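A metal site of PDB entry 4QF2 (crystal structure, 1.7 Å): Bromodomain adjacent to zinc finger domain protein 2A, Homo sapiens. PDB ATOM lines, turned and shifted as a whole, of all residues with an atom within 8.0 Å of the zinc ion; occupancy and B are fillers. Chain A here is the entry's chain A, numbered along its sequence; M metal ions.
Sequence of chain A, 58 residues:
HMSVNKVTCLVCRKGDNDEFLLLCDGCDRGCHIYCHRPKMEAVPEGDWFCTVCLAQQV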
ATOM      1  N   LEU A  10      24.319 -11.893  21.117  1.00  0.00           N
ATOM      2  CA  LEU A  10      23.262 -11.150  20.412  1.00  0.00           C
ATOM      3  C   LEU A  10      23.344 -11.173  18.890  1.00  0.00           C
ATOM      4  O   LEU A  10      22.317 -11.105  18.229  1.00  0.00           O
ATOM      5  CB  LEU A  10      23.231  -9.694  20.859  1.00  0.00           C
ATOM      6  CG  LEU A  10      22.611  -9.376  22.194  1.00  0.00           C
ATOM      7  CD1 LEU A  10      22.881  -7.906  22.523  1.00  0.00           C
ATOM      8  CD2 LEU A  10      21.114  -9.657  22.194  1.00  0.00           C
ATOM      9  N   LEU A  23      29.937  -9.764  28.580  1.00  0.00           N
ATOM     10  CA  LEU A  23      28.677  -9.849  29.320  1.00  0.00           C
ATOM     11  C   LEU A  23      28.222  -8.449  29.710  1.00  0.00           C
ATOM     12  O   LEU A  23      29.034  -7.646  30.217  1.00  0.00           O
ATOM     13  CB  LEU A  23      28.868 -10.697  30.584  1.00  0.00           C
ATOM     14  CG  LEU A  23      29.417 -12.101  30.315  1.00  0.00           C
ATOM     15  CD1 LEU A  23      29.751 -12.834  31.619  1.00  0.00           C
ATOM     16  CD2 LEU A  23      28.375 -12.857  29.506  1.00  0.00           C
ATOM     17  N   CYS A  24      26.960  -8.147  29.400  1.00  0.00           N
ATOM     18  CA  CYS A  24      26.410  -6.810  29.624  1.00  0.00           C
ATOM     19  C   CYS A  24      26.268  -6.583  31.106  1.00  0.00           C
ATOM     20  O   CYS A  24      25.779  -7.453  31.829  1.00  0.00           O
ATOM     21  CB  CYS A  24      25.030  -6.630  28.966  1.00  0.00           C
ATOM     22  SG  CYS A  24      24.322  -4.970  29.130  1.00  0.00           S
ATOM     23  N   ASP A  25      26.676  -5.410  31.540  1.00  0.00           N
ATOM     24  CA  ASP A  25      26.528  -5.011  32.951  1.00  0.00           C
ATOM     25  C   ASP A  25      25.129  -4.487  33.317  1.00  0.00           C
ATOM     26  O   ASP A  25      24.815  -4.302  34.515  1.00  0.00           O
ATOM     27  CB  ASP A  25      27.618  -4.035  33.255  1.00  0.00           C
ATOM     28  CG  ASP A  25      28.980  -4.708  33.316  1.00  0.00           C
ATOM     29  OD1 ASP A  25      29.133  -5.695  34.060  1.00  0.00           O
ATOM     30  OD2 ASP A  25      29.900  -4.281  32.591  1.00  0.00           O
ATOM     31  N   GLY A  26      24.286  -4.296  32.313  1.00  0.00           N
ATOM     32  CA  GLY A  26      22.909  -3.847  32.503  1.00  0.00           C
ATOM     33  C   GLY A  26      21.809  -4.899  32.392  1.00  0.00           C
ATOM     34  O   GLY A  26      20.645  -4.604  32.737  1.00  0.00           O
ATOM     35  N   CYS A  27      22.126  -6.089  31.885  1.00  0.00           N
ATOM     36  CA  CYS A  27      21.144  -7.134  31.677  1.00  0.00           C
ATOM     37  C   CYS A  27      21.940  -8.418  31.509  1.00  0.00           C
ATOM     38  O   CYS A  27      23.156  -8.453  31.781  1.00  0.00           O
ATOM     39  CB  CYS A  27      20.240  -6.834  30.480  1.00  0.00           C
ATOM     40  SG  CYS A  27      21.110  -6.913  28.878  1.00  0.00           S
ATOM     41  N   ASP A  28      21.260  -9.477  31.075  1.00  0.00           N
ATOM     42  CA  ASP A  28      21.887 -10.783  30.934  1.00  0.00           C
ATOM     43  C   ASP A  28      22.247 -11.089  29.492  1.00  0.00           C
ATOM     44  O   ASP A  28      22.493 -12.255  29.165  1.00  0.00           O
ATOM     45  CB  ASP A  28      20.968 -11.879  31.536  1.00  0.00           C
ATOM     46  CG  ASP A  28      19.653 -12.039  30.795  1.00  0.00           C
ATOM     47  OD1 ASP A  28      19.204 -11.063  30.145  1.00  0.00           O
ATOM     48  OD2 ASP A  28      19.068 -13.133  30.884  1.00  0.00           O
ATOM     49  N   ARG A  29      22.305 -10.053  28.650  1.00  0.00           N
ATOM     50  CA  ARG A  29      22.684 -10.254  27.247  1.00  0.00           C
ATOM     51  C   ARG A  29      24.185 -10.325  27.082  1.00  0.00           C
ATOM     52  O   ARG A  29      24.976  -9.924  27.960  1.00  0.00           O
ATOM     53  CB  ARG A  29      22.101  -9.167  26.338  1.00  0.00           C
ATOM     54  CG  ARG A  29      20.592  -9.175  26.263  1.00  0.00           C
ATOM     55  CD  ARG A  29      20.049  -8.044  25.420  1.00  0.00           C
ATOM     56  NE  ARG A  29      18.595  -8.100  25.400  1.00  0.00           N
ATOM     57  CZ  ARG A  29      17.824  -7.602  26.365  1.00  0.00           C
ATOM     58  NH1 ARG A  29      18.365  -7.014  27.429  1.00  0.00           N
ATOM     59  NH2 ARG A  29      16.505  -7.703  26.273  1.00  0.00           N
ATOM     60  N   GLY A  30      24.608 -10.911  25.961  1.00  0.00           N
ATOM     61  CA  GLY A  30      26.047 -11.054  25.689  1.00  0.00           C
ATOM     62  C   GLY A  30      26.417 -10.845  24.255  1.00  0.00           C
ATOM     63  O   GLY A  30      25.554 -10.688  23.391  1.00  0.00           O
ATOM     64  N   TRP A  48      30.737  -2.896  30.090  1.00  0.00           N
ATOM     65  CA  TRP A  48      30.273  -2.946  28.711  1.00  0.00           C
ATOM     66  C   TRP A  48      28.739  -3.038  28.722  1.00  0.00           C
ATOM     67  O   TRP A  48      28.145  -3.782  29.521  1.00  0.00           O
ATOM     68  CB  TRP A  48      30.916  -4.077  27.920  1.00  0.00           C
ATOM     69  CG  TRP A  48      30.356  -4.190  26.552  1.00  0.00           C
ATOM     70  CD1 TRP A  48      30.676  -3.413  25.481  1.00  0.00           C
ATOM     71  CD2 TRP A  48      29.339  -5.085  26.119  1.00  0.00           C
ATOM     72  NE1 TRP A  48      29.918  -3.779  24.409  1.00  0.00           N
ATOM     73  CE2 TRP A  48      29.096  -4.807  24.764  1.00  0.00           C
ATOM     74  CE3 TRP A  48      28.600  -6.099  26.742  1.00  0.00           C
ATOM     75  CZ2 TRP A  48      28.163  -5.488  24.036  1.00  0.00           C
ATOM     76  CZ3 TRP A  48      27.681  -6.812  25.985  1.00  0.00           C
ATOM     77  CH2 TRP A  48      27.484  -6.495  24.654  1.00  0.00           C
ATOM     78  N   PHE A  49      28.100  -2.219  27.876  1.00  0.00           N
ATOM     79  CA  PHE A  49      26.655  -2.271  27.732  1.00  0.00           C
ATOM     80  C   PHE A  49      26.269  -2.662  26.336  1.00  0.00           C
ATOM     81  O   PHE A  49      26.844  -2.173  25.327  1.00  0.00           O
ATOM     82  CB  PHE A  49      25.950  -0.979  28.149  1.00  0.00           C
ATOM     83  CG  PHE A  49      26.165  -0.630  29.582  1.00  0.00           C
ATOM     84  CD1 PHE A  49      25.381  -1.213  30.566  1.00  0.00           C
ATOM     85  CD2 PHE A  49      27.200   0.199  29.958  1.00  0.00           C
ATOM     86  CE1 PHE A  49      25.592  -0.912  31.901  1.00  0.00           C
ATOM     87  CE2 PHE A  49      27.421   0.499  31.282  1.00  0.00           C
ATOM     88  CZ  PHE A  49      26.624  -0.078  32.263  1.00  0.00           C
ATOM     89  N   CYS A  50      25.329  -3.573  26.284  1.00  0.00           N
ATOM     90  CA  CYS A  50      24.728  -3.985  25.072  1.00  0.00           C
ATOM     91  C   CYS A  50      23.842  -2.877  24.530  1.00  0.00           C
ATOM     92  O   CYS A  50      23.518  -1.909  25.210  1.00  0.00           O
ATOM     93  CB  CYS A  50      23.899  -5.239  25.270  1.00  0.00           C
ATOM     94  SG  CYS A  50      22.261  -4.973  26.000  1.00  0.00           S
ATOM     95  N   THR A  51      23.438  -3.033  23.277  1.00  0.00           N
ATOM     96  CA  THR A  51      22.609  -2.058  22.608  1.00  0.00           C
ATOM     97  C   THR A  51      21.230  -1.825  23.201  1.00  0.00           C
ATOM     98  O   THR A  51      20.690  -0.739  23.078  1.00  0.00           O
ATOM     99  CB  THR A  51      22.571  -2.367  21.105  1.00  0.00           C
ATOM    100  OG1 THR A  51      22.299  -3.751  20.911  1.00  0.00           O
ATOM    101  CG2 THR A  51      23.929  -2.067  20.480  1.00  0.00           C
ATOM    102  N   VAL A  52      20.649  -2.840  23.830  1.00  0.00           N
ATOM    103  CA  VAL A  52      19.349  -2.719  24.473  1.00  0.00           C
ATOM    104  C   VAL A  52      19.503  -1.779  25.659  1.00  0.00           C
ATOM    105  O   VAL A  52      18.683  -0.857  25.858  1.00  0.00           O
ATOM    106  CB  VAL A  52      18.842  -4.072  24.939  1.00  0.00           C
ATOM    107  CG1 VAL A  52      17.584  -3.894  25.798  1.00  0.00           C
ATOM    108  CG2 VAL A  52      18.619  -4.997  23.737  1.00  0.00           C
ATOM    109  N   CYS A  53      20.549  -2.005  26.439  1.00  0.00           N
ATOM    110  CA  CYS A  53      20.880  -1.103  27.560  1.00  0.00           C
ATOM    111  C   CYS A  53      21.302   0.319  27.131  1.00  0.00           C
ATOM    112  O   CYS A  53      20.943   1.301  27.816  1.00  0.00           O
ATOM    113  CB  CYS A  53      21.937  -1.747  28.428  1.00  0.00           C
ATOM    114  SG  CYS A  53      21.285  -3.181  29.349  1.00  0.00           S
ATOM    115  N   LEU A  54      22.072   0.459  26.049  1.00  0.00           N
ATOM    116  CA  LEU A  54      22.397   1.800  25.540  1.00  0.00           C
ATOM    117  C   LEU A  54      21.134   2.561  25.199  1.00  0.00           C
ATOM    118  O   LEU A  54      21.017   3.785  25.383  1.00  0.00           O
ATOM    119  CB  LEU A  54      23.290   1.697  24.292  1.00  0.00           C
ATOM    120  CG  LEU A  54      24.746   1.291  24.533  1.00  0.00           C
ATOM    121  CD1 LEU A  54      25.479   1.109  23.208  1.00  0.00           C
ATOM    122  CD2 LEU A  54      25.450   2.332  25.407  1.00  0.00           C
ATOM    123  N   GLN A  56      18.387   2.525  26.791  1.00  0.00           N
ATOM    124  CA  GLN A  56      17.757   3.015  28.032  1.00  0.00           C
ATOM    125  C   GLN A  56      18.453   4.246  28.650  1.00  0.00           C
ATOM    126  O   GLN A  56      17.917   4.894  29.568  1.00  0.00           O
ATOM    127  CB  GLN A  56      17.774   1.906  29.084  1.00  0.00           C
ATOM    128  CG  GLN A  56      16.985   0.672  28.726  1.00  0.00           C
ATOM    129  CD  GLN A  56      15.510   0.991  28.683  1.00  0.00           C
ATOM    130  OE1 GLN A  56      14.937   1.070  27.612  1.00  0.00           O
ATOM    131  NE2 GLN A  56      14.907   1.264  29.860  1.00  0.00           N
HETATM  132 ZN    ZN M   1      22.275  -5.040  28.350  1.00  0.00          ZN
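The zinc ion is bound by the side-chain sulfur (SG) of Cys 24 (2.2 Å), the side-chain sulfur (SG) of Cys 27 (2.3 Å), the side-chain sulfur (SG) of Cys 53 (2.3 Å) and the side-chain sulfur (SG) of Cys 50 (2.4 Å). The zinc ion has four donor atoms within binding distance.
Of the 17 residues printed, 4 come within 4 Å of the zinc ion. The nearest printed residue that does not touch the zinc ion is Gly 26 (4.1 Å).
SG of Cys 24 sits close to N of Gly 26, at 3.3 Å. The backbone NH of Cys 24 is in hydrogen-bond range of the backbone carbonyl oxygen of Arg 29. The guanidinium group of Arg 29 sits close to the side-chain sulfur of Cys 27 (3.1 Å). The side-chain sulfur of Cys 53 sits close to the backbone carbonyl oxygen of Gly 26, 3.7 Å away. The backbone NH (N) of Val 52 lies close to the side-chain sulfur (SG) of Cys 50, at 3.4 Å.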
